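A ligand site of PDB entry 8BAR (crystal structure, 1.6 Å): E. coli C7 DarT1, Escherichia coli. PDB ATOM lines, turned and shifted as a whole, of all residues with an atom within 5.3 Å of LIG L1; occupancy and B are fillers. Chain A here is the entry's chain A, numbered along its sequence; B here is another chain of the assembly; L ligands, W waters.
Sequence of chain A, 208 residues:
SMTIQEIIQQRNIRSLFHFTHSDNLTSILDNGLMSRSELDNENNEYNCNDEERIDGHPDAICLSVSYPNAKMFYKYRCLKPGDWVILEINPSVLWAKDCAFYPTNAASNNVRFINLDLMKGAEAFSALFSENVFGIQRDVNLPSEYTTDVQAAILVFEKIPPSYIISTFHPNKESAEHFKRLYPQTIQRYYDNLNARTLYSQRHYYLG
Water W8 lies within hydrogen-bond range of an oxygen (O8) of LIG L1 (2.5 Å) and a nitrogen (N2) of LG2 L2 (2.6 Å). Water W2 bridges O6 of LIG L1 and N of Cys 62. Water W3 lies within hydrogen-bond range of an oxygen (O13) of LIG L1, the backbone carbonyl oxygen of Ala 60 and the guanidinium group of Arg 53. Water W4 lies within hydrogen-bond range of O2 of LIG L1, O of Phe 19, ND2 of Asn 49 and N2 of LG2 L2. Water W1 lies within hydrogen-bond range of O2 of LIG L1 (2.9 Å), O of Asn 47 (3.0 Å), OD1 of Asn 49 (3.1 Å), N of His 21 (3.1 Å) and ND2 of Asn 24 (3.4 Å). Water W7 lies within hydrogen-bond range of N of Ala 106 (3.0 Å), OD1 of Asn 105 (3.3 Å) and SG of Cys 62 (3.4 Å).
The backbone carbonyl oxygen (O) of Cys 62 lies within hydrogen-bond range of a ring nitrogen (ND1) of His 18, at 2.8 Å. The backbone NH of Asn 47 sits at hydrogen-bond distance from the side-chain amide oxygen of Asn 24 (2.9 Å). OD2 of Asp 55 lies within salt-bridge range of NH2 of Arg 53 (2.9 Å). OD1 of Asn 105 lies within hydrogen-bond range of N of Ala 107 (3.0 Å). The side-chain sulfur (SG) of Cys 48 sits close to the guanidinium group (NH1) of Arg 36. The guanidinium group (NH1) of Arg 36 lies within hydrogen-bond range of the backbone carbonyl oxygen (O) of Asp 50. The backbone carbonyl oxygen of Ser 27 sits at hydrogen-bond distance from the side-chain amide nitrogen of Asn 31, 3.0 Å away. The side-chain amide nitrogen (ND2) of Asn 24 sits at hydrogen-bond distance from the side-chain hydroxyl (OG1) of Thr 20.
ND1 of His 18 sits at hydrogen-bond distance from N2 of LG2 L2 (3.4 Å). An oxygen (O5) of LIG L1 is in salt-bridge range of the guanidinium group of Arg 36 (2.8 Å). N of Phe 19 sits at hydrogen-bond distance from O1 of LG2 L2, at 2.9 Å. N1 of LG2 L2 lies close to SG of Cys 62, at 3.3 Å. An oxygen (O2) of LIG L1 lies within hydrogen-bond range of the backbone carbonyl oxygen (O) of Asn 47. A ring nitrogen (NE2) of His 18 is in hydrogen-bond range of an oxygen (O1) of LIG L1, at 2.7 Å. N2 of DG 3 of chain B is bonded to a carbon (C12) of LIG L1 (1.4 Å). O of Gly 32 lies within hydrogen-bond range of N3 of LIG L1, at 2.9 Å. N of Asp 50 sits at hydrogen-bond distance from O9 of LIG L1 (2.9 Å). An oxygen (O12) of LIG L1 is in hydrogen-bond range of the backbone NH (N) of Ala 107 (3.4 Å). The side-chain amide nitrogen of Asn 49 sits at hydrogen-bond distance from an oxygen (O8) of LIG L1 (2.9 Å). OG1 of Thr 20 sits at hydrogen-bond distance from O1 of LIG L1, at 2.6 Å. OG of Ser 27 is in hydrogen-bond range of N1 of LIG L1 (2.6 Å). OD1 of Asp 55 sits at hydrogen-bond distance from O12 of LIG L1, 2.9 Å away. N2 of LG2 L2 is in hydrogen-bond range of O of Phe 19. N of Met 34 sits at hydrogen-bond distance from N4 of LIG L1 (3.0 Å). The backbone NH (N) of Asn 49 lies within hydrogen-bond range of an oxygen (O9) of LIG L1, 2.9 Å away. NH1 of Arg 53 lies within salt-bridge range of O5 of LIG L1 (2.9 Å). O2 of LIG L1 is in hydrogen-bond range of ND2 of Asn 24 (3.5 Å).
CG1 of Ile 28 touches C3 of LIG L1, 3.4 Å away. Leu 33 touches LIG L1 (CA to N4, 3.5 Å). Leu 39 touches LIG L1. Glu 45 touches LIG L1. Tyr 46 touches LIG L1. Cys 48 touches LIG L1. CB of Cys 62 touches C14 of LIG L1 (3.98 Å). Met 72 touches LIG L1 (CE to O11, 3.5 Å). Asn 105 touches LIG L1. Ala 106 touches LIG L1. Leu 155 touches LIG L1 (CD2 to O13, 3.9 Å).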
ATOM      1  N   HIS A  18     -14.650  -0.591  -2.537  1.00  0.00           N
ATOM      2  CA  HIS A  18     -13.974   0.691  -2.747  1.00  0.00           C
ATOM      3  C   HIS A  18     -14.307   1.579  -1.559  1.00  0.00           C
ATOM      4  O   HIS A  18     -15.470   1.937  -1.337  1.00  0.00           O
ATOM      5  CB  HIS A  18     -14.478   1.353  -4.030  1.00  0.00           C
ATOM      6  CG  HIS A  18     -13.924   2.690  -4.359  1.00  0.00           C
ATOM      7  ND1 HIS A  18     -12.805   2.878  -5.129  1.00  0.00           N
ATOM      8  CD2 HIS A  18     -14.356   3.921  -3.997  1.00  0.00           C
ATOM      9  CE1 HIS A  18     -12.597   4.204  -5.233  1.00  0.00           C
ATOM     10  NE2 HIS A  18     -13.548   4.856  -4.554  1.00  0.00           N
ATOM     11  N   PHE A  19     -13.287   1.915  -0.759  1.00  0.00           N
ATOM     12  CA  PHE A  19     -13.504   2.853   0.343  1.00  0.00           C
ATOM     13  C   PHE A  19     -13.409   4.269  -0.184  1.00  0.00           C
ATOM     14  O   PHE A  19     -12.664   4.545  -1.113  1.00  0.00           O
ATOM     15  CB  PHE A  19     -12.531   2.609   1.501  1.00  0.00           C
ATOM     16  CG  PHE A  19     -11.075   2.832   1.182  1.00  0.00           C
ATOM     17  CD1 PHE A  19     -10.501   4.098   1.196  1.00  0.00           C
ATOM     18  CD2 PHE A  19     -10.293   1.758   0.832  1.00  0.00           C
ATOM     19  CE1 PHE A  19      -9.153   4.251   0.923  1.00  0.00           C
ATOM     20  CE2 PHE A  19      -8.947   1.931   0.558  1.00  0.00           C
ATOM     21  CZ  PHE A  19      -8.366   3.179   0.613  1.00  0.00           C
ATOM     22  N   THR A  20     -14.117   5.196   0.475  1.00  0.00           N
ATOM     23  CA  THR A  20     -14.068   6.599   0.055  1.00  0.00           C
ATOM     24  C   THR A  20     -14.624   7.434   1.203  1.00  0.00           C
ATOM     25  O   THR A  20     -15.440   6.955   1.976  1.00  0.00           O
ATOM     26  CB  THR A  20     -14.854   6.820  -1.247  1.00  0.00           C
ATOM     27  OG1 THR A  20     -14.524   8.088  -1.798  1.00  0.00           O
ATOM     28  CG2 THR A  20     -16.344   6.629  -1.086  1.00  0.00           C
ATOM     29  N   HIS A  21     -14.291   8.706   1.237  1.00  0.00           N
ATOM     30  CA  HIS A  21     -14.798   9.612   2.265  1.00  0.00           C
ATOM     31  C   HIS A  21     -16.275   9.815   1.966  1.00  0.00           C
ATOM     32  O   HIS A  21     -16.639   9.941   0.797  1.00  0.00           O
ATOM     33  CB  HIS A  21     -13.965  10.905   2.266  1.00  0.00           C
ATOM     34  CG  HIS A  21     -14.220  11.682   3.500  1.00  0.00           C
ATOM     35  ND1 HIS A  21     -15.370  12.442   3.665  1.00  0.00           N
ATOM     36  CD2 HIS A  21     -13.499  11.804   4.646  1.00  0.00           C
ATOM     37  CE1 HIS A  21     -15.328  12.978   4.891  1.00  0.00           C
ATOM     38  NE2 HIS A  21     -14.215  12.574   5.514  1.00  0.00           N
ATOM     39  N   ASN A  24     -17.793  12.219  -0.746  1.00  0.00           N
ATOM     40  CA  ASN A  24     -17.901  11.824  -2.140  1.00  0.00           C
ATOM     41  C   ASN A  24     -19.160  11.032  -2.470  1.00  0.00           C
ATOM     42  O   ASN A  24     -19.431  10.816  -3.648  1.00  0.00           O
ATOM     43  CB  ASN A  24     -16.708  10.952  -2.528  1.00  0.00           C
ATOM     44  CG  ASN A  24     -15.399  11.714  -2.385  1.00  0.00           C
ATOM     45  OD1 ASN A  24     -15.364  12.908  -2.685  1.00  0.00           O
ATOM     46  ND2 ASN A  24     -14.334  10.999  -1.987  1.00  0.00           N
ATOM     47  N   SER A  27     -22.214  12.179  -4.866  1.00  0.00           N
ATOM     48  CA  SER A  27     -21.776  12.303  -6.255  1.00  0.00           C
ATOM     49  C   SER A  27     -21.585  10.920  -6.884  1.00  0.00           C
ATOM     50  O   SER A  27     -21.848  10.714  -8.074  1.00  0.00           O
ATOM     51  CB  SER A  27     -20.509  13.146  -6.301  1.00  0.00           C
ATOM     52  OG  SER A  27     -19.995  13.229  -7.608  1.00  0.00           O
ATOM     53  N   ILE A  28     -21.077   9.955  -6.116  1.00  0.00           N
ATOM     54  CA  ILE A  28     -20.881   8.596  -6.605  1.00  0.00           C
ATOM     55  C   ILE A  28     -22.238   7.907  -6.826  1.00  0.00           C
ATOM     56  O   ILE A  28     -22.397   7.204  -7.829  1.00  0.00           O
ATOM     57  CB  ILE A  28     -19.987   7.776  -5.637  1.00  0.00           C
ATOM     58  CG1 ILE A  28     -18.555   8.276  -5.611  1.00  0.00           C
ATOM     59  CG2 ILE A  28     -20.051   6.322  -6.011  1.00  0.00           C
ATOM     60  CD1 ILE A  28     -17.740   7.755  -4.402  1.00  0.00           C
ATOM     61  N   ASN A  31     -23.655   9.527  -9.996  1.00  0.00           N
ATOM     62  CA  ASN A  31     -22.941   9.581 -11.266  1.00  0.00           C
ATOM     63  C   ASN A  31     -22.149   8.319 -11.530  1.00  0.00           C
ATOM     64  O   ASN A  31     -21.582   8.152 -12.612  1.00  0.00           O
ATOM     65  CB  ASN A  31     -21.940  10.750 -11.311  1.00  0.00           C
ATOM     66  CG  ASN A  31     -22.567  12.107 -11.111  1.00  0.00           C
ATOM     67  OD1 ASN A  31     -23.517  12.436 -11.792  1.00  0.00           O
ATOM     68  ND2 ASN A  31     -22.032  12.908 -10.178  1.00  0.00           N
ATOM     69  N   GLY A  32     -22.055   7.448 -10.522  1.00  0.00           N
ATOM     70  CA  GLY A  32     -21.163   6.290 -10.631  1.00  0.00           C
ATOM     71  C   GLY A  32     -19.757   6.677 -10.184  1.00  0.00           C
ATOM     72  O   GLY A  32     -19.461   7.850  -9.960  1.00  0.00           O
ATOM     73  N   LEU A  33     -18.880   5.675 -10.054  1.00  0.00           N
ATOM     74  CA  LEU A  33     -17.472   5.966  -9.826  1.00  0.00           C
ATOM     75  C   LEU A  33     -16.823   6.456 -11.103  1.00  0.00           C
ATOM     76  O   LEU A  33     -17.034   5.886 -12.176  1.00  0.00           O
ATOM     77  CB  LEU A  33     -16.786   4.691  -9.340  1.00  0.00           C
ATOM     78  CG  LEU A  33     -17.057   4.264  -7.910  1.00  0.00           C
ATOM     79  CD1 LEU A  33     -16.494   2.869  -7.687  1.00  0.00           C
ATOM     80  CD2 LEU A  33     -16.383   5.231  -6.949  1.00  0.00           C
ATOM     81  N   MET A  34     -15.962   7.464 -10.954  1.00  0.00           N
ATOM     82  CA  MET A  34     -15.184   7.981 -12.067  1.00  0.00           C
ATOM     83  C   MET A  34     -13.721   8.081 -11.637  1.00  0.00           C
ATOM     84  O   MET A  34     -13.415   8.261 -10.451  1.00  0.00           O
ATOM     85  CB  MET A  34     -15.699   9.376 -12.467  1.00  0.00           C
ATOM     86  CG  MET A  34     -17.071   9.281 -13.060  1.00  0.00           C
ATOM     87  SD  MET A  34     -17.750  10.950 -13.490  1.00  0.00           S
ATOM     88  CE  MET A  34     -18.494  11.422 -11.963  1.00  0.00           C
ATOM     89  N   ARG A  36      -9.956   9.833 -11.400  1.00  0.00           N
ATOM     90  CA  ARG A  36      -9.443  11.179 -11.169  1.00  0.00           C
ATOM     91  C   ARG A  36      -9.418  12.026 -12.453  1.00  0.00           C
ATOM     92  O   ARG A  36      -9.874  13.166 -12.428  1.00  0.00           O
ATOM     93  CB  ARG A  36      -8.054  11.136 -10.553  1.00  0.00           C
ATOM     94  CG  ARG A  36      -7.642  12.499  -9.988  1.00  0.00           C
ATOM     95  CD  ARG A  36      -6.281  12.504  -9.319  1.00  0.00           C
ATOM     96  NE  ARG A  36      -6.309  11.705  -8.097  1.00  0.00           N
ATOM     97  CZ  ARG A  36      -5.530  11.931  -7.052  1.00  0.00           C
ATOM     98  NH1 ARG A  36      -5.549  11.118  -6.012  1.00  0.00           N
ATOM     99  NH2 ARG A  36      -4.759  13.005  -7.076  1.00  0.00           N
ATOM    100  N   LEU A  39     -13.020  12.930 -13.371  1.00  0.00           N
ATOM    101  CA  LEU A  39     -13.611  13.905 -12.476  1.00  0.00           C
ATOM    102  C   LEU A  39     -13.064  15.302 -12.806  1.00  0.00           C
ATOM    103  O   LEU A  39     -13.811  16.280 -12.809  1.00  0.00           O
ATOM    104  CB  LEU A  39     -13.299  13.529 -11.039  1.00  0.00           C
ATOM    105  CG  LEU A  39     -14.002  12.271 -10.544  1.00  0.00           C
ATOM    106  CD1 LEU A  39     -13.331  11.716  -9.296  1.00  0.00           C
ATOM    107  CD2 LEU A  39     -15.465  12.569 -10.262  1.00  0.00           C
ATOM    108  N   GLU A  45     -16.469  17.995  -8.146  1.00  0.00           N
ATOM    109  CA  GLU A  45     -15.790  18.095  -6.873  1.00  0.00           C
ATOM    110  C   GLU A  45     -15.541  16.685  -6.349  1.00  0.00           C
ATOM    111  O   GLU A  45     -16.408  15.819  -6.442  1.00  0.00           O
ATOM    112  CB  GLU A  45     -16.636  18.896  -5.890  1.00  0.00           C
ATOM    113  CG  GLU A  45     -16.094  18.924  -4.476  1.00  0.00           C
ATOM    114  CD  GLU A  45     -16.854  19.883  -3.559  1.00  0.00           C
ATOM    115  OE1 GLU A  45     -17.660  20.693  -4.084  1.00  0.00           O
ATOM    116  OE2 GLU A  45     -16.640  19.813  -2.333  1.00  0.00           O
ATOM    117  N   TYR A  46     -14.370  16.489  -5.740  1.00  0.00           N
ATOM    118  CA  TYR A  46     -14.099  15.225  -5.083  1.00  0.00           C
ATOM    119  C   TYR A  46     -13.032  15.440  -4.013  1.00  0.00           C
ATOM    120  O   TYR A  46     -12.255  16.383  -4.092  1.00  0.00           O
ATOM    121  CB  TYR A  46     -13.657  14.181  -6.098  1.00  0.00           C
ATOM    122  CG  TYR A  46     -12.397  14.494  -6.850  1.00  0.00           C
ATOM    123  CD1 TYR A  46     -12.417  15.250  -8.004  1.00  0.00           C
ATOM    124  CD2 TYR A  46     -11.153  14.039  -6.433  1.00  0.00           C
ATOM    125  CE1 TYR A  46     -11.260  15.554  -8.703  1.00  0.00           C
ATOM    126  CE2 TYR A  46      -9.991  14.335  -7.101  1.00  0.00           C
ATOM    127  CZ  TYR A  46     -10.033  15.108  -8.254  1.00  0.00           C
ATOM    128  OH  TYR A  46      -8.864  15.404  -8.943  1.00  0.00           O
ATOM    129  N   ASN A  47     -13.060  14.556  -3.019  1.00  0.00           N
ATOM    130  CA  ASN A  47     -12.058  14.503  -1.962  1.00  0.00           C
ATOM    131  C   ASN A  47     -11.188  13.279  -2.217  1.00  0.00           C
ATOM    132  O   ASN A  47     -11.646  12.151  -2.008  1.00  0.00           O
ATOM    133  CB  ASN A  47     -12.777  14.369  -0.628  1.00  0.00           C
ATOM    134  CG  ASN A  47     -11.874  14.471   0.578  1.00  0.00           C
ATOM    135  OD1 ASN A  47     -10.661  14.602   0.423  1.00  0.00           O
ATOM    136  ND2 ASN A  47     -12.473  14.587   1.767  1.00  0.00           N
ATOM    137  N   CYS A  48      -9.953  13.496  -2.690  1.00  0.00           N
ATOM    138  CA  CYS A  48      -9.063  12.386  -2.941  1.00  0.00           C
ATOM    139  C   CYS A  48      -8.093  12.161  -1.783  1.00  0.00           C
ATOM    140  O   CYS A  48      -8.022  12.965  -0.833  1.00  0.00           O
ATOM    141  CB  CYS A  48      -8.315  12.553  -4.250  1.00  0.00           C
ATOM    142  SG  CYS A  48      -7.181  13.947  -4.269  1.00  0.00           S
ATOM    143  N   ASN A  49      -7.351  11.050  -1.845  1.00  0.00           N
ATOM    144  CA  ASN A  49      -6.436  10.636  -0.793  1.00  0.00           C
ATOM    145  C   ASN A  49      -4.979  10.827  -1.212  1.00  0.00           C
ATOM    146  O   ASN A  49      -4.162  11.451  -0.509  1.00  0.00           O
ATOM    147  CB  ASN A  49      -6.751   9.194  -0.420  1.00  0.00           C
ATOM    148  CG  ASN A  49      -8.228   8.987  -0.169  1.00  0.00           C
ATOM    149  OD1 ASN A  49      -8.799   9.731   0.621  1.00  0.00           O
ATOM    150  ND2 ASN A  49      -8.802   7.979  -0.778  1.00  0.00           N
ATOM    151  N   ASP A  50      -4.678  10.267  -2.389  1.00  0.00           N
ATOM    152  CA  ASP A  50      -3.333  10.133  -2.914  1.00  0.00           C
ATOM    153  C   ASP A  50      -2.921  11.447  -3.577  1.00  0.00           C
ATOM    154  O   ASP A  50      -3.658  11.954  -4.431  1.00  0.00           O
ATOM    155  CB  ASP A  50      -3.324   8.935  -3.869  1.00  0.00           C
ATOM    156  CG  ASP A  50      -1.957   8.451  -4.334  1.00  0.00           C
ATOM    157  OD1 ASP A  50      -0.993   9.257  -4.240  1.00  0.00           O
ATOM    158  OD2 ASP A  50      -1.857   7.324  -4.830  1.00  0.00           O
ATOM    159  N   ARG A  53      -0.071   9.470  -6.933  1.00  0.00           N
ATOM    160  CA  ARG A  53      -0.527   8.554  -7.973  1.00  0.00           C
ATOM    161  C   ARG A  53       0.668   7.937  -8.703  1.00  0.00           C
ATOM    162  O   ARG A  53       0.758   7.977  -9.956  1.00  0.00           O
ATOM    163  CB  ARG A  53      -1.526   9.285  -8.884  1.00  0.00           C
ATOM    164  CG  ARG A  53      -2.890   9.571  -8.231  1.00  0.00           C
ATOM    165  CD  ARG A  53      -3.512   8.365  -7.617  1.00  0.00           C
ATOM    166  NE  ARG A  53      -3.782   7.270  -8.532  1.00  0.00           N
ATOM    167  CZ  ARG A  53      -4.796   7.195  -9.392  1.00  0.00           C
ATOM    168  NH1 ARG A  53      -5.836   8.024  -9.354  1.00  0.00           N
ATOM    169  NH2 ARG A  53      -4.749   6.253 -10.321  1.00  0.00           N
ATOM    170  N   ASP A  55       1.182   4.860  -9.240  1.00  0.00           N
ATOM    171  CA  ASP A  55       0.691   3.832 -10.161  1.00  0.00           C
ATOM    172  C   ASP A  55       0.782   4.321 -11.611  1.00  0.00           C
ATOM    173  O   ASP A  55       0.938   3.501 -12.539  1.00  0.00           O
ATOM    174  CB  ASP A  55      -0.729   3.392  -9.808  1.00  0.00           C
ATOM    175  CG  ASP A  55      -1.662   4.594  -9.746  1.00  0.00           C
ATOM    176  OD1 ASP A  55      -1.636   5.345  -8.708  1.00  0.00           O
ATOM    177  OD2 ASP A  55      -2.298   4.856 -10.796  1.00  0.00           O
ATOM    178  N   ALA A  60      -7.778   5.510 -14.094  1.00  0.00           N
ATOM    179  CA  ALA A  60      -8.317   4.270 -13.569  1.00  0.00           C
ATOM    180  C   ALA A  60      -8.806   4.424 -12.123  1.00  0.00           C
ATOM    181  O   ALA A  60      -8.175   5.102 -11.328  1.00  0.00           O
ATOM    182  CB  ALA A  60      -7.287   3.188 -13.657  1.00  0.00           C
ATOM    183  N   ILE A  61      -9.941   3.750 -11.857  1.00  0.00           N
ATOM    184  CA  ILE A  61     -10.566   3.666 -10.547  1.00  0.00           C
ATOM    185  C   ILE A  61      -9.978   2.446  -9.839  1.00  0.00           C
ATOM    186  O   ILE A  61      -9.825   1.421 -10.476  1.00  0.00           O
ATOM    187  CB  ILE A  61     -12.074   3.456 -10.705  1.00  0.00           C
ATOM    188  CG1 ILE A  61     -12.703   4.651 -11.437  1.00  0.00           C
ATOM    189  CG2 ILE A  61     -12.763   3.246  -9.362  1.00  0.00           C
ATOM    190  CD1 ILE A  61     -14.015   4.329 -12.130  1.00  0.00           C
ATOM    191  N   CYS A  62      -9.668   2.539  -8.520  1.00  0.00           N
ATOM    192  CA  CYS A  62      -9.063   1.401  -7.848  1.00  0.00           C
ATOM    193  C   CYS A  62     -10.087   0.692  -6.979  1.00  0.00           C
ATOM    194  O   CYS A  62     -10.752   1.316  -6.143  1.00  0.00           O
ATOM    195  CB  CYS A  62      -7.867   1.855  -7.014  1.00  0.00           C
ATOM    196  SG  CYS A  62      -6.871   0.464  -6.411  1.00  0.00           S
ATOM    197  N   MET A  72      -3.993   1.005   3.568  1.00  0.00           N
ATOM    198  CA  MET A  72      -4.153   2.354   3.055  1.00  0.00           C
ATOM    199  C   MET A  72      -5.411   3.012   3.641  1.00  0.00           C
ATOM    200  O   MET A  72      -5.424   4.195   3.993  1.00  0.00           O
ATOM    201  CB  MET A  72      -4.187   2.365   1.526  1.00  0.00           C
ATOM    202  CG  MET A  72      -4.414   3.736   0.981  1.00  0.00           C
ATOM    203  SD  MET A  72      -4.474   3.617  -0.853  1.00  0.00           S
ATOM    204  CE  MET A  72      -5.205   5.213  -1.203  1.00  0.00           C
ATOM    205  N   ASN A 105      -0.502  -3.522  -4.162  1.00  0.00           N
ATOM    206  CA  ASN A 105      -0.826  -2.144  -4.433  1.00  0.00           C
ATOM    207  C   ASN A 105      -0.303  -1.750  -5.823  1.00  0.00           C
ATOM    208  O   ASN A 105       0.852  -2.040  -6.127  1.00  0.00           O
ATOM    209  CB  ASN A 105      -0.162  -1.305  -3.326  1.00  0.00           C
ATOM    210  CG  ASN A 105      -0.646   0.126  -3.217  1.00  0.00           C
ATOM    211  OD1 ASN A 105      -0.684   0.863  -4.207  1.00  0.00           O
ATOM    212  ND2 ASN A 105      -0.910   0.580  -1.991  1.00  0.00           N
ATOM    213  N   ALA A 106      -1.151  -1.113  -6.649  1.00  0.00           N
ATOM    214  CA  ALA A 106      -0.827  -0.760  -8.042  1.00  0.00           C
ATOM    215  C   ALA A 106       0.296   0.280  -8.108  1.00  0.00           C
ATOM    216  O   ALA A 106       0.963   0.395  -9.143  1.00  0.00           O
ATOM    217  CB  ALA A 106      -2.071  -0.241  -8.734  1.00  0.00           C
ATOM    218  N   ALA A 107       0.575   0.958  -6.977  1.00  0.00           N
ATOM    219  CA  ALA A 107       1.695   1.900  -6.908  1.00  0.00           C
ATOM    220  C   ALA A 107       3.020   1.241  -6.564  1.00  0.00           C
ATOM    221  O   ALA A 107       4.045   1.930  -6.565  1.00  0.00           O
ATOM    222  CB  ALA A 107       1.383   3.027  -5.922  1.00  0.00           C
ATOM    223  N   LEU A 155      -7.485  -2.055 -11.225  1.00  0.00           N
ATOM    224  CA  LEU A 155      -7.610  -0.754 -11.821  1.00  0.00           C
ATOM    225  C   LEU A 155      -8.610  -0.845 -12.985  1.00  0.00           C
ATOM    226  O   LEU A 155      -8.449  -1.674 -13.882  1.00  0.00           O
ATOM    227  CB  LEU A 155      -6.263  -0.224 -12.279  1.00  0.00           C
ATOM    228  CG  LEU A 155      -5.301   0.263 -11.186  1.00  0.00           C
ATOM    229  CD1 LEU A 155      -4.064   0.828 -11.843  1.00  0.00           C
ATOM    230  CD2 LEU A 155      -5.906   1.308 -10.262  1.00  0.00           C
ATOM    231  P    DG B   3       1.415   3.063   5.335  1.00  0.00           P
ATOM    232  OP1  DG B   3       2.195   1.855   5.736  1.00  0.00           O
ATOM    233  OP2  DG B   3       2.042   4.385   4.937  1.00  0.00           O
ATOM    234  O5'  DG B   3       0.404   2.799   4.108  1.00  0.00           O
ATOM    235  C5'  DG B   3      -0.171   1.498   3.894  1.00  0.00           C
ATOM    236  C4'  DG B   3       0.163   1.027   2.488  1.00  0.00           C
ATOM    237  O4'  DG B   3      -0.491   1.882   1.530  1.00  0.00           O
ATOM    238  C3'  DG B   3       1.657   1.083   2.170  1.00  0.00           C
ATOM    239  O3'  DG B   3       1.950  -0.034   1.287  1.00  0.00           O
ATOM    240  C2'  DG B   3       1.798   2.419   1.469  1.00  0.00           C
ATOM    241  C1'  DG B   3       0.496   2.507   0.700  1.00  0.00           C
ATOM    242  N9   DG B   3       0.014   3.860   0.448  1.00  0.00           N
ATOM    243  C8   DG B   3       0.010   4.916   1.328  1.00  0.00           C
ATOM    244  N7   DG B   3      -0.591   5.989   0.880  1.00  0.00           N
ATOM    245  C5   DG B   3      -0.991   5.616  -0.408  1.00  0.00           C
ATOM    246  C6   DG B   3      -1.677   6.357  -1.399  1.00  0.00           C
ATOM    247  O6   DG B   3      -2.091   7.522  -1.339  1.00  0.00           O
ATOM    248  N1   DG B   3      -1.934   5.560  -2.528  1.00  0.00           N
ATOM    249  C2   DG B   3      -1.560   4.247  -2.698  1.00  0.00           C
ATOM    250  N2   DG B   3      -1.940   3.598  -3.807  1.00  0.00           N
ATOM    251  N3   DG B   3      -0.906   3.552  -1.766  1.00  0.00           N
ATOM    252  C4   DG B   3      -0.640   4.309  -0.677  1.00  0.00           C
HETATM  253  N1  LIG L   1     -17.796  11.805  -7.294  1.00  0.00           N
HETATM  254  C1  LIG L   1     -16.924  12.118  -6.325  1.00  0.00           C
HETATM  255  N2  LIG L   1     -15.818  11.488  -5.935  1.00  0.00           N
HETATM  256  C2  LIG L   1     -15.636  10.363  -6.663  1.00  0.00           C
HETATM  257  C3  LIG L   1     -16.423   9.915  -7.709  1.00  0.00           C
HETATM  258  C4  LIG L   1     -17.555  10.696  -8.030  1.00  0.00           C
HETATM  259  N3  LIG L   1     -18.441  10.372  -8.957  1.00  0.00           N
HETATM  260  N4  LIG L   1     -15.923   8.718  -8.221  1.00  0.00           N
HETATM  261  C5  LIG L   1     -14.820   8.496  -7.533  1.00  0.00           C
HETATM  262  N5  LIG L   1     -14.620   9.465  -6.554  1.00  0.00           N
HETATM  263  C6  LIG L   1     -13.563   9.557  -5.579  1.00  0.00           C
HETATM  264  C7  LIG L   1     -12.948   8.233  -5.134  1.00  0.00           C
HETATM  265  O1  LIG L   1     -13.773   7.484  -4.248  1.00  0.00           O
HETATM  266  C8  LIG L   1     -11.649   8.703  -4.505  1.00  0.00           C
HETATM  267  O2  LIG L   1     -11.759   8.966  -3.099  1.00  0.00           O
HETATM  268  O3  LIG L   1     -12.474  10.260  -6.102  1.00  0.00           O
HETATM  269  C9  LIG L   1     -11.348  10.025  -5.235  1.00  0.00           C
HETATM  270  C10 LIG L   1     -10.023  10.145  -5.958  1.00  0.00           C
HETATM  271  O4  LIG L   1      -9.826   9.070  -6.770  1.00  0.00           O
HETATM  272  P1  LIG L   1      -8.436   8.347  -6.845  1.00  0.00           P
HETATM  273  O5  LIG L   1      -7.267   9.235  -7.143  1.00  0.00           O
HETATM  274  O6  LIG L   1      -8.772   7.224  -7.822  1.00  0.00           O
HETATM  275  O7  LIG L   1      -8.253   7.656  -5.391  1.00  0.00           O
HETATM  276  P2  LIG L   1      -7.114   7.750  -4.255  1.00  0.00           P
HETATM  277  O8  LIG L   1      -7.700   6.808  -3.231  1.00  0.00           O
HETATM  278  O9  LIG L   1      -6.789   9.187  -3.984  1.00  0.00           O
HETATM  279  O10 LIG L   1      -5.850   7.069  -4.962  1.00  0.00           O
HETATM  280  C11 LIG L   1      -5.969   5.669  -5.410  1.00  0.00           C
HETATM  281  O11 LIG L   1      -3.848   4.935  -4.447  1.00  0.00           O
HETATM  282  C12 LIG L   1      -2.666   4.233  -4.870  1.00  0.00           C
HETATM  283  O12 LIG L   1      -2.117   3.064  -6.963  1.00  0.00           O
HETATM  284  C13 LIG L   1      -3.113   3.266  -5.959  1.00  0.00           C
HETATM  285  O13 LIG L   1      -4.556   4.059  -7.836  1.00  0.00           O
HETATM  286  C14 LIG L   1      -4.456   3.820  -6.438  1.00  0.00           C
HETATM  287  C15 LIG L   1      -4.566   5.154  -5.696  1.00  0.00           C
HETATM  288  N1  LG2 L   2      -6.965  -0.074  -3.194  1.00  0.00           N
HETATM  289  C1  LG2 L   2      -8.235   0.312  -3.000  1.00  0.00           C
HETATM  290  C2  LG2 L   2      -8.656   1.638  -2.956  1.00  0.00           C
HETATM  291  C3  LG2 L   2      -7.682   2.629  -3.122  1.00  0.00           C
HETATM  292  C4  LG2 L   2      -6.363   2.258  -3.313  1.00  0.00           C
HETATM  293  C5  LG2 L   2      -6.057   0.902  -3.332  1.00  0.00           C
HETATM  294  C6  LG2 L   2     -10.095   2.008  -2.670  1.00  0.00           C
HETATM  295  O1  LG2 L   2     -10.842   1.148  -2.214  1.00  0.00           O
HETATM  296  N2  LG2 L   2     -10.468   3.277  -2.690  1.00  0.00           N
HETATM  297  O   HOH W   1     -11.752   9.657  -0.272  1.00  0.00           O
HETATM  298  O   HOH W   2      -9.864   5.047  -7.054  1.00  0.00           O
HETATM  299  O   HOH W   3      -6.979   4.814  -8.683  1.00  0.00           O
HETATM  300  O   HOH W   4     -11.076   6.577  -2.079  1.00  0.00           O
HETATM  301  O   HOH W   5      -8.489   7.556 -10.349  1.00  0.00           O
HETATM  302  O   HOH W   6     -11.872   7.140  -8.444  1.00  0.00           O
HETATM  303  O   HOH W   7      -3.619  -0.061  -5.393  1.00  0.00           O
HETATM  304  O   HOH W   8      -9.462   5.247  -4.136  1.00  0.00           O
